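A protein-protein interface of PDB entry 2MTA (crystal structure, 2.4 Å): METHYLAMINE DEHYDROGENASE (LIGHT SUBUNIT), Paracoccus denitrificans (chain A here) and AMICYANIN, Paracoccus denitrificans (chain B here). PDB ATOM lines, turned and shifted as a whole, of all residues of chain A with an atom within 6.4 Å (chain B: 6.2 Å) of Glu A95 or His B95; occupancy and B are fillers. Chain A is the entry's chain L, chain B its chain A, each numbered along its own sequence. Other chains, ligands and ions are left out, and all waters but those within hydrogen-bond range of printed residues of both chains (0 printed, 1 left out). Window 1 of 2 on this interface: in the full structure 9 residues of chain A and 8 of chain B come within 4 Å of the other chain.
CE3 of TRQ A51 is covalently linked to CD1 of Trp A102, 1.4 Å away.
The backbone NH of Val A52 lies within hydrogen-bond range of the backbone carbonyl oxygen of Glu A95 (3.2 Å).
N of Leu A89 sits at hydrogen-bond distance from O of Phe A96, 3.3 Å away.
The side-chain carboxylate (OE2) of Glu A95 is in salt-bridge range of the guanidinium group (NH2) of Arg A93.
O of Ala A97 sits at hydrogen-bond distance from NE1 of Trp A102, at 3.0 Å.
Ser A50 touches Pro B94.
CE of Met B51 touches CG2 of Val A52 (3.8 Å).
Phe B97 touches Pro A94 (CE1 to CG, 3.5 Å).
Met B51 touches Glu A95.
His B95 touches Glu A95.
Phe B97 touches Glu A95.
Phe A96 touches Met B51 (CZ to CE, 3.8 Å).
O of Pro B94 touches CH2 of Trp A102 (3.7 Å).
Printed residues of chain B within 4 Å of Ser A50: Pro B94 (3.9 Å).
Of the printed residues of chain B, Val A52 touches Met B51.
Of the printed residues of chain B, Pro A94 touches Phe B97 (3.5 Å).
Printed residues of chain B within 4 Å of Trp A102: Pro B94 (3.7 Å).
Of the printed residues of chain A, Met B51 touches Val A52, Glu A95 and Phe A96.
Of chain A, only Glu A95 comes within 4 Å of His B95.
The nearest residue of chain B that does not touch Glu A95 is Met B28 (4.1 Å).
The nearest residue of chain A that does not touch His B95 is Ser A50 (4.7 Å).
Of the 14 printed residues of chain A, 6 touch a printed residue of chain B.
Printed residues of chain A that touch a printed residue of chain B: Ser A50, Val A52, Pro A94, Glu A95, Phe A96 and Trp A102.
Along chain A the printed residues that touch a printed residue of chain B span positions 50 to 102.
Among the printed residues, 8 pairs touch across the chains.
Among the printed residues, no Asp or Glu carboxylate lies within 4 Å of a Lys or Arg side-chain nitrogen of the other chain.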
ATOM      1  N   SER A  50     -16.218 -28.630 -21.576  1.00  0.00           N
ATOM      2  CA  SER A  50     -16.714 -29.977 -21.724  1.00  0.00           C
ATOM      3  C   SER A  50     -16.967 -30.459 -23.136  1.00  0.00           C
ATOM      4  O   SER A  50     -17.059 -29.621 -24.027  1.00  0.00           O
ATOM      5  CB  SER A  50     -18.026 -30.120 -20.943  1.00  0.00           C
ATOM      6  OG  SER A  50     -18.811 -28.896 -20.974  1.00  0.00           O
ATOM      7  N   TRQ A  51     -16.986 -31.788 -23.330  1.00  0.00           N
ATOM      8  CA  TRQ A  51     -17.556 -32.338 -24.533  1.00  0.00           C
ATOM      9  C   TRQ A  51     -19.030 -32.470 -24.228  1.00  0.00           C
ATOM     10  O   TRQ A  51     -19.365 -32.357 -23.048  1.00  0.00           O
ATOM     11  CB  TRQ A  51     -17.005 -33.714 -24.886  1.00  0.00           C
ATOM     12  CG  TRQ A  51     -16.988 -34.896 -23.908  1.00  0.00           C
ATOM     13  CD1 TRQ A  51     -17.971 -35.866 -24.029  1.00  0.00           C
ATOM     14  NE1 TRQ A  51     -17.736 -36.716 -23.082  1.00  0.00           N
ATOM     15  CE2 TRQ A  51     -16.665 -36.310 -22.378  1.00  0.00           C
ATOM     16  CZ2 TRQ A  51     -16.200 -37.026 -21.268  1.00  0.00           C
ATOM     17  CH2 TRQ A  51     -15.086 -36.472 -20.658  1.00  0.00           C
ATOM     18  CZ3 TRQ A  51     -14.467 -35.356 -21.153  1.00  0.00           C
ATOM     19  CE3 TRQ A  51     -14.939 -34.651 -22.209  1.00  0.00           C
ATOM     20  CD2 TRQ A  51     -16.080 -35.119 -22.892  1.00  0.00           C
ATOM     21  O6  TRQ A  51     -14.630 -36.958 -19.615  1.00  0.00           O
ATOM     22  O7  TRQ A  51     -16.852 -37.982 -20.790  1.00  0.00           O
ATOM     23  N   VAL A  52     -19.959 -32.639 -25.161  1.00  0.00           N
ATOM     24  CA  VAL A  52     -21.353 -32.803 -24.826  1.00  0.00           C
ATOM     25  C   VAL A  52     -21.865 -34.026 -25.536  1.00  0.00           C
ATOM     26  O   VAL A  52     -21.117 -34.670 -26.259  1.00  0.00           O
ATOM     27  CB  VAL A  52     -22.270 -31.577 -25.213  1.00  0.00           C
ATOM     28  CG1 VAL A  52     -21.777 -30.293 -24.545  1.00  0.00           C
ATOM     29  CG2 VAL A  52     -22.304 -31.404 -26.687  1.00  0.00           C
ATOM     30  N   ALA A  53     -23.113 -34.414 -25.300  1.00  0.00           N
ATOM     31  CA  ALA A  53     -23.833 -35.514 -25.927  1.00  0.00           C
ATOM     32  C   ALA A  53     -25.316 -35.205 -25.758  1.00  0.00           C
ATOM     33  O   ALA A  53     -25.651 -34.322 -24.963  1.00  0.00           O
ATOM     34  CB  ALA A  53     -23.614 -36.856 -25.240  1.00  0.00           C
ATOM     35  N   LEU A  89     -17.882 -38.110 -31.953  1.00  0.00           N
ATOM     36  CA  LEU A  89     -17.204 -37.738 -33.189  1.00  0.00           C
ATOM     37  C   LEU A  89     -15.670 -37.576 -33.022  1.00  0.00           C
ATOM     38  O   LEU A  89     -15.227 -37.344 -31.878  1.00  0.00           O
ATOM     39  CB  LEU A  89     -17.920 -36.445 -33.648  1.00  0.00           C
ATOM     40  CG  LEU A  89     -18.952 -36.391 -34.786  1.00  0.00           C
ATOM     41  CD1 LEU A  89     -19.953 -37.531 -34.789  1.00  0.00           C
ATOM     42  CD2 LEU A  89     -19.682 -35.086 -34.626  1.00  0.00           C
ATOM     43  N   VAL A  91     -11.473 -36.376 -33.103  1.00  0.00           N
ATOM     44  CA  VAL A  91     -10.934 -35.208 -32.410  1.00  0.00           C
ATOM     45  C   VAL A  91     -11.047 -33.942 -33.255  1.00  0.00           C
ATOM     46  O   VAL A  91     -11.059 -32.863 -32.671  1.00  0.00           O
ATOM     47  CB  VAL A  91      -9.471 -35.466 -32.023  1.00  0.00           C
ATOM     48  CG1 VAL A  91      -8.684 -35.588 -33.302  1.00  0.00           C
ATOM     49  CG2 VAL A  91      -8.808 -34.333 -31.231  1.00  0.00           C
ATOM     50  N   TYR A  92     -11.184 -34.039 -34.599  1.00  0.00           N
ATOM     51  CA  TYR A  92     -11.237 -32.831 -35.379  1.00  0.00           C
ATOM     52  C   TYR A  92     -12.597 -32.237 -35.190  1.00  0.00           C
ATOM     53  O   TYR A  92     -12.778 -31.126 -35.639  1.00  0.00           O
ATOM     54  CB  TYR A  92     -10.948 -33.111 -36.862  1.00  0.00           C
ATOM     55  CG  TYR A  92     -11.882 -34.069 -37.583  1.00  0.00           C
ATOM     56  CD1 TYR A  92     -13.055 -33.590 -38.155  1.00  0.00           C
ATOM     57  CD2 TYR A  92     -11.544 -35.400 -37.697  1.00  0.00           C
ATOM     58  CE1 TYR A  92     -13.893 -34.453 -38.843  1.00  0.00           C
ATOM     59  CE2 TYR A  92     -12.377 -36.267 -38.397  1.00  0.00           C
ATOM     60  CZ  TYR A  92     -13.547 -35.787 -38.961  1.00  0.00           C
ATOM     61  OH  TYR A  92     -14.364 -36.679 -39.648  1.00  0.00           O
ATOM     62  N   ARG A  93     -13.548 -32.910 -34.550  1.00  0.00           N
ATOM     63  CA  ARG A  93     -14.774 -32.260 -34.164  1.00  0.00           C
ATOM     64  C   ARG A  93     -14.749 -32.143 -32.653  1.00  0.00           C
ATOM     65  O   ARG A  93     -15.469 -32.901 -32.022  1.00  0.00           O
ATOM     66  CB  ARG A  93     -15.968 -33.054 -34.550  1.00  0.00           C
ATOM     67  CG  ARG A  93     -16.152 -33.234 -36.062  1.00  0.00           C
ATOM     68  CD  ARG A  93     -16.252 -31.878 -36.767  1.00  0.00           C
ATOM     69  NE  ARG A  93     -17.423 -31.143 -36.298  1.00  0.00           N
ATOM     70  CZ  ARG A  93     -18.696 -31.454 -36.661  1.00  0.00           C
ATOM     71  NH1 ARG A  93     -19.016 -32.458 -37.515  1.00  0.00           N
ATOM     72  NH2 ARG A  93     -19.708 -30.814 -36.064  1.00  0.00           N
ATOM     73  N   PRO A  94     -13.999 -31.252 -31.959  1.00  0.00           N
ATOM     74  CA  PRO A  94     -13.798 -31.355 -30.511  1.00  0.00           C
ATOM     75  C   PRO A  94     -15.026 -31.250 -29.587  1.00  0.00           C
ATOM     76  O   PRO A  94     -15.181 -31.973 -28.615  1.00  0.00           O
ATOM     77  CB  PRO A  94     -12.752 -30.322 -30.269  1.00  0.00           C
ATOM     78  CG  PRO A  94     -12.650 -29.386 -31.449  1.00  0.00           C
ATOM     79  CD  PRO A  94     -13.072 -30.297 -32.568  1.00  0.00           C
ATOM     80  N   GLU A  95     -16.028 -30.477 -29.904  1.00  0.00           N
ATOM     81  CA  GLU A  95     -17.220 -30.347 -29.113  1.00  0.00           C
ATOM     82  C   GLU A  95     -17.962 -31.653 -28.866  1.00  0.00           C
ATOM     83  O   GLU A  95     -18.779 -31.695 -27.950  1.00  0.00           O
ATOM     84  CB  GLU A  95     -18.159 -29.290 -29.790  1.00  0.00           C
ATOM     85  CG  GLU A  95     -18.758 -29.492 -31.191  1.00  0.00           C
ATOM     86  CD  GLU A  95     -17.883 -29.469 -32.452  1.00  0.00           C
ATOM     87  OE1 GLU A  95     -16.666 -29.352 -32.452  1.00  0.00           O
ATOM     88  OE2 GLU A  95     -18.459 -29.588 -33.508  1.00  0.00           O
ATOM     89  N   PHE A  96     -17.791 -32.762 -29.591  1.00  0.00           N
ATOM     90  CA  PHE A  96     -18.490 -34.049 -29.316  1.00  0.00           C
ATOM     91  C   PHE A  96     -17.523 -35.199 -29.094  1.00  0.00           C
ATOM     92  O   PHE A  96     -17.898 -36.360 -29.206  1.00  0.00           O
ATOM     93  CB  PHE A  96     -19.348 -34.502 -30.474  1.00  0.00           C
ATOM     94  CG  PHE A  96     -20.388 -33.471 -30.864  1.00  0.00           C
ATOM     95  CD1 PHE A  96     -21.471 -33.213 -30.047  1.00  0.00           C
ATOM     96  CD2 PHE A  96     -20.220 -32.795 -32.045  1.00  0.00           C
ATOM     97  CE1 PHE A  96     -22.381 -32.268 -30.432  1.00  0.00           C
ATOM     98  CE2 PHE A  96     -21.149 -31.844 -32.419  1.00  0.00           C
ATOM     99  CZ  PHE A  96     -22.233 -31.574 -31.618  1.00  0.00           C
ATOM    100  N   ALA A  97     -16.245 -34.854 -28.893  1.00  0.00           N
ATOM    101  CA  ALA A  97     -15.151 -35.818 -28.795  1.00  0.00           C
ATOM    102  C   ALA A  97     -14.871 -36.172 -27.330  1.00  0.00           C
ATOM    103  O   ALA A  97     -14.709 -35.304 -26.448  1.00  0.00           O
ATOM    104  CB  ALA A  97     -13.906 -35.250 -29.371  1.00  0.00           C
ATOM    105  N   ILE A 100     -10.648 -36.547 -25.053  1.00  0.00           N
ATOM    106  CA  ILE A 100      -9.947 -35.383 -24.606  1.00  0.00           C
ATOM    107  C   ILE A 100     -10.202 -35.214 -23.099  1.00  0.00           C
ATOM    108  O   ILE A 100     -11.355 -35.301 -22.638  1.00  0.00           O
ATOM    109  CB  ILE A 100     -10.465 -34.111 -25.310  1.00  0.00           C
ATOM    110  CG1 ILE A 100     -10.245 -34.314 -26.814  1.00  0.00           C
ATOM    111  CG2 ILE A 100      -9.810 -32.839 -24.730  1.00  0.00           C
ATOM    112  CD1 ILE A 100     -10.769 -33.217 -27.810  1.00  0.00           C
ATOM    113  N   TRP A 102     -11.201 -33.129 -20.603  1.00  0.00           N
ATOM    114  CA  TRP A 102     -11.951 -31.929 -20.398  1.00  0.00           C
ATOM    115  C   TRP A 102     -11.738 -31.313 -19.048  1.00  0.00           C
ATOM    116  O   TRP A 102     -12.695 -31.159 -18.303  1.00  0.00           O
ATOM    117  CB  TRP A 102     -13.422 -32.253 -20.642  1.00  0.00           C
ATOM    118  CG  TRP A 102     -13.663 -32.514 -22.113  1.00  0.00           C
ATOM    119  CD1 TRP A 102     -14.172 -33.631 -22.830  1.00  0.00           C
ATOM    120  CD2 TRP A 102     -13.284 -31.603 -23.099  1.00  0.00           C
ATOM    121  NE1 TRP A 102     -14.139 -33.442 -24.158  1.00  0.00           N
ATOM    122  CE2 TRP A 102     -13.588 -32.207 -24.330  1.00  0.00           C
ATOM    123  CE3 TRP A 102     -12.713 -30.312 -23.034  1.00  0.00           C
ATOM    124  CZ2 TRP A 102     -13.311 -31.494 -25.517  1.00  0.00           C
ATOM    125  CZ3 TRP A 102     -12.449 -29.609 -24.208  1.00  0.00           C
ATOM    126  CH2 TRP A 102     -12.752 -30.214 -25.434  1.00  0.00           C
ATOM    127  N   MET B  28     -22.099 -22.352 -33.626  1.00  0.00           N
ATOM    128  CA  MET B  28     -20.669 -22.484 -33.332  1.00  0.00           C
ATOM    129  C   MET B  28     -19.874 -21.273 -33.728  1.00  0.00           C
ATOM    130  O   MET B  28     -18.693 -21.394 -34.074  1.00  0.00           O
ATOM    131  CB  MET B  28     -20.109 -23.717 -34.019  1.00  0.00           C
ATOM    132  CG  MET B  28     -20.716 -25.059 -33.575  1.00  0.00           C
ATOM    133  SD  MET B  28     -20.324 -25.559 -31.873  1.00  0.00           S
ATOM    134  CE  MET B  28     -18.570 -25.441 -31.997  1.00  0.00           C
ATOM    135  N   MET B  51     -25.495 -25.607 -26.780  1.00  0.00           N
ATOM    136  CA  MET B  51     -24.078 -25.940 -26.676  1.00  0.00           C
ATOM    137  C   MET B  51     -23.479 -24.859 -25.808  1.00  0.00           C
ATOM    138  O   MET B  51     -23.668 -23.679 -26.124  1.00  0.00           O
ATOM    139  CB  MET B  51     -23.526 -25.906 -28.070  1.00  0.00           C
ATOM    140  CG  MET B  51     -22.043 -25.988 -28.372  1.00  0.00           C
ATOM    141  SD  MET B  51     -21.369 -27.622 -28.041  1.00  0.00           S
ATOM    142  CE  MET B  51     -22.128 -28.638 -29.283  1.00  0.00           C
ATOM    143  N   PRO B  52     -22.874 -25.188 -24.675  1.00  0.00           N
ATOM    144  CA  PRO B  52     -22.314 -24.147 -23.829  1.00  0.00           C
ATOM    145  C   PRO B  52     -21.074 -23.551 -24.480  1.00  0.00           C
ATOM    146  O   PRO B  52     -20.247 -24.240 -25.085  1.00  0.00           O
ATOM    147  CB  PRO B  52     -22.099 -24.870 -22.486  1.00  0.00           C
ATOM    148  CG  PRO B  52     -23.152 -25.954 -22.546  1.00  0.00           C
ATOM    149  CD  PRO B  52     -22.997 -26.464 -23.981  1.00  0.00           C
ATOM    150  N   HIS B  53     -20.876 -22.250 -24.357  1.00  0.00           N
ATOM    151  CA  HIS B  53     -19.731 -21.548 -24.944  1.00  0.00           C
ATOM    152  C   HIS B  53     -19.280 -20.473 -23.983  1.00  0.00           C
ATOM    153  O   HIS B  53     -20.119 -19.989 -23.243  1.00  0.00           O
ATOM    154  CB  HIS B  53     -20.062 -20.780 -26.283  1.00  0.00           C
ATOM    155  CG  HIS B  53     -20.522 -21.590 -27.499  1.00  0.00           C
ATOM    156  ND1 HIS B  53     -19.721 -22.467 -28.054  1.00  0.00           N
ATOM    157  CD2 HIS B  53     -21.794 -21.603 -28.010  1.00  0.00           C
ATOM    158  CE1 HIS B  53     -20.468 -23.085 -28.936  1.00  0.00           C
ATOM    159  NE2 HIS B  53     -21.673 -22.574 -28.890  1.00  0.00           N
ATOM    160  N   ASN B  54     -18.054 -19.960 -24.076  1.00  0.00           N
ATOM    161  CA  ASN B  54     -17.626 -18.871 -23.210  1.00  0.00           C
ATOM    162  C   ASN B  54     -16.793 -17.897 -24.014  1.00  0.00           C
ATOM    163  O   ASN B  54     -16.782 -18.030 -25.234  1.00  0.00           O
ATOM    164  CB  ASN B  54     -16.793 -19.426 -22.062  1.00  0.00           C
ATOM    165  CG  ASN B  54     -15.411 -19.946 -22.380  1.00  0.00           C
ATOM    166  OD1 ASN B  54     -15.102 -20.513 -23.447  1.00  0.00           O
ATOM    167  ND2 ASN B  54     -14.537 -19.777 -21.384  1.00  0.00           N
ATOM    168  N   MET B  71     -18.858 -20.391 -18.320  1.00  0.00           N
ATOM    169  CA  MET B  71     -19.558 -20.927 -19.460  1.00  0.00           C
ATOM    170  C   MET B  71     -20.963 -20.407 -19.436  1.00  0.00           C
ATOM    171  O   MET B  71     -21.531 -20.249 -18.355  1.00  0.00           O
ATOM    172  CB  MET B  71     -19.588 -22.422 -19.442  1.00  0.00           C
ATOM    173  CG  MET B  71     -18.164 -22.961 -19.734  1.00  0.00           C
ATOM    174  SD  MET B  71     -17.350 -22.806 -21.382  1.00  0.00           S
ATOM    175  CE  MET B  71     -18.282 -23.978 -22.289  1.00  0.00           C
ATOM    176  N   HIS B  91     -11.062 -16.368 -27.911  1.00  0.00           N
ATOM    177  CA  HIS B  91     -11.580 -17.601 -28.490  1.00  0.00           C
ATOM    178  C   HIS B  91     -12.477 -18.270 -27.467  1.00  0.00           C
ATOM    179  O   HIS B  91     -12.721 -17.727 -26.397  1.00  0.00           O
ATOM    180  CB  HIS B  91     -10.471 -18.529 -28.823  1.00  0.00           C
ATOM    181  CG  HIS B  91      -9.754 -19.086 -27.592  1.00  0.00           C
ATOM    182  ND1 HIS B  91      -8.925 -18.406 -26.818  1.00  0.00           N
ATOM    183  CD2 HIS B  91      -9.902 -20.384 -27.127  1.00  0.00           C
ATOM    184  CE1 HIS B  91      -8.560 -19.245 -25.893  1.00  0.00           C
ATOM    185  NE2 HIS B  91      -9.141 -20.422 -26.076  1.00  0.00           N
ATOM    186  N   CYS B  92     -13.018 -19.440 -27.705  1.00  0.00           N
ATOM    187  CA  CYS B  92     -13.879 -20.122 -26.817  1.00  0.00           C
ATOM    188  C   CYS B  92     -13.051 -21.245 -26.271  1.00  0.00           C
ATOM    189  O   CYS B  92     -12.650 -22.109 -27.016  1.00  0.00           O
ATOM    190  CB  CYS B  92     -14.968 -20.680 -27.558  1.00  0.00           C
ATOM    191  SG  CYS B  92     -16.147 -21.477 -26.424  1.00  0.00           S
ATOM    192  N   THR B  93     -12.885 -21.360 -24.982  1.00  0.00           N
ATOM    193  CA  THR B  93     -12.102 -22.398 -24.321  1.00  0.00           C
ATOM    194  C   THR B  93     -12.361 -23.832 -24.775  1.00  0.00           C
ATOM    195  O   THR B  93     -11.365 -24.455 -25.161  1.00  0.00           O
ATOM    196  CB  THR B  93     -12.362 -22.224 -22.795  1.00  0.00           C
ATOM    197  OG1 THR B  93     -12.262 -20.821 -22.422  1.00  0.00           O
ATOM    198  CG2 THR B  93     -11.392 -23.026 -22.031  1.00  0.00           C
ATOM    199  N   PRO B  94     -13.556 -24.463 -24.818  1.00  0.00           N
ATOM    200  CA  PRO B  94     -13.645 -25.835 -25.294  1.00  0.00           C
ATOM    201  C   PRO B  94     -13.530 -26.026 -26.795  1.00  0.00           C
ATOM    202  O   PRO B  94     -13.352 -27.105 -27.348  1.00  0.00           O
ATOM    203  CB  PRO B  94     -14.975 -26.348 -24.748  1.00  0.00           C
ATOM    204  CG  PRO B  94     -15.805 -25.101 -24.653  1.00  0.00           C
ATOM    205  CD  PRO B  94     -14.797 -24.037 -24.198  1.00  0.00           C
ATOM    206  N   HIS B  95     -13.668 -24.906 -27.495  1.00  0.00           N
ATOM    207  CA  HIS B  95     -13.824 -24.879 -28.975  1.00  0.00           C
ATOM    208  C   HIS B  95     -12.900 -23.813 -29.596  1.00  0.00           C
ATOM    209  O   HIS B  95     -13.435 -22.789 -30.034  1.00  0.00           O
ATOM    210  CB  HIS B  95     -15.317 -24.581 -29.289  1.00  0.00           C
ATOM    211  CG  HIS B  95     -16.330 -25.460 -28.542  1.00  0.00           C
ATOM    212  ND1 HIS B  95     -17.366 -24.910 -27.983  1.00  0.00           N
ATOM    213  CD2 HIS B  95     -16.389 -26.815 -28.479  1.00  0.00           C
ATOM    214  CE1 HIS B  95     -18.133 -25.861 -27.554  1.00  0.00           C
ATOM    215  NE2 HIS B  95     -17.537 -26.984 -27.856  1.00  0.00           N
ATOM    216  N   PRO B  96     -11.550 -23.919 -29.646  1.00  0.00           N
ATOM    217  CA  PRO B  96     -10.656 -22.840 -30.002  1.00  0.00           C
ATOM    218  C   PRO B  96     -10.679 -22.441 -31.476  1.00  0.00           C
ATOM    219  O   PRO B  96     -10.029 -21.492 -31.873  1.00  0.00           O
ATOM    220  CB  PRO B  96      -9.311 -23.310 -29.495  1.00  0.00           C
ATOM    221  CG  PRO B  96      -9.340 -24.778 -29.593  1.00  0.00           C
ATOM    222  CD  PRO B  96     -10.793 -25.146 -29.375  1.00  0.00           C
ATOM    223  N   PHE B  97     -11.435 -23.115 -32.340  1.00  0.00           N
ATOM    224  CA  PHE B  97     -11.696 -22.644 -33.697  1.00  0.00           C
ATOM    225  C   PHE B  97     -12.772 -21.546 -33.678  1.00  0.00           C
ATOM    226  O   PHE B  97     -13.128 -21.004 -34.729  1.00  0.00           O
ATOM    227  CB  PHE B  97     -12.189 -23.811 -34.610  1.00  0.00           C
ATOM    228  CG  PHE B  97     -13.313 -24.605 -33.990  1.00  0.00           C
ATOM    229  CD1 PHE B  97     -12.989 -25.668 -33.176  1.00  0.00           C
ATOM    230  CD2 PHE B  97     -14.650 -24.236 -34.174  1.00  0.00           C
ATOM    231  CE1 PHE B  97     -14.020 -26.355 -32.543  1.00  0.00           C
ATOM    232  CE2 PHE B  97     -15.664 -24.932 -33.533  1.00  0.00           C
ATOM    233  CZ  PHE B  97     -15.349 -26.000 -32.707  1.00  0.00           C
ATOM    234  N   MET B  98     -13.393 -21.222 -32.533  1.00  0.00           N
ATOM    235  CA  MET B  98     -14.391 -20.148 -32.469  1.00  0.00           C
ATOM    236  C   MET B  98     -13.630 -18.908 -32.009  1.00  0.00           C
ATOM    237  O   MET B  98     -13.120 -18.907 -30.893  1.00  0.00           O
ATOM    238  CB  MET B  98     -15.458 -20.477 -31.456  1.00  0.00           C
ATOM    239  CG  MET B  98     -16.423 -21.508 -31.934  1.00  0.00           C
ATOM    240  SD  MET B  98     -17.770 -21.572 -30.719  1.00  0.00           S
ATOM    241  CE  MET B  98     -18.166 -19.883 -30.389  1.00  0.00           C
ATOM    242  N   ARG B  99     -13.476 -17.858 -32.811  1.00  0.00           N
ATOM    243  CA  ARG B  99     -12.688 -16.674 -32.475  1.00  0.00           C
ATOM    244  C   ARG B  99     -13.413 -15.383 -32.773  1.00  0.00           C
ATOM    245  O   ARG B  99     -14.400 -15.374 -33.511  1.00  0.00           O
ATOM    246  CB  ARG B  99     -11.410 -16.658 -33.238  1.00  0.00           C
ATOM    247  CG  ARG B  99     -10.531 -17.819 -32.818  1.00  0.00           C
ATOM    248  CD  ARG B  99      -9.194 -17.876 -33.525  1.00  0.00           C
ATOM    249  NE  ARG B  99      -9.314 -18.738 -34.670  1.00  0.00           N
ATOM    250  CZ  ARG B  99      -8.754 -19.947 -34.744  1.00  0.00           C
ATOM    251  NH1 ARG B  99      -8.029 -20.550 -33.793  1.00  0.00           N
ATOM    252  NH2 ARG B  99      -9.054 -20.625 -35.821  1.00  0.00           N
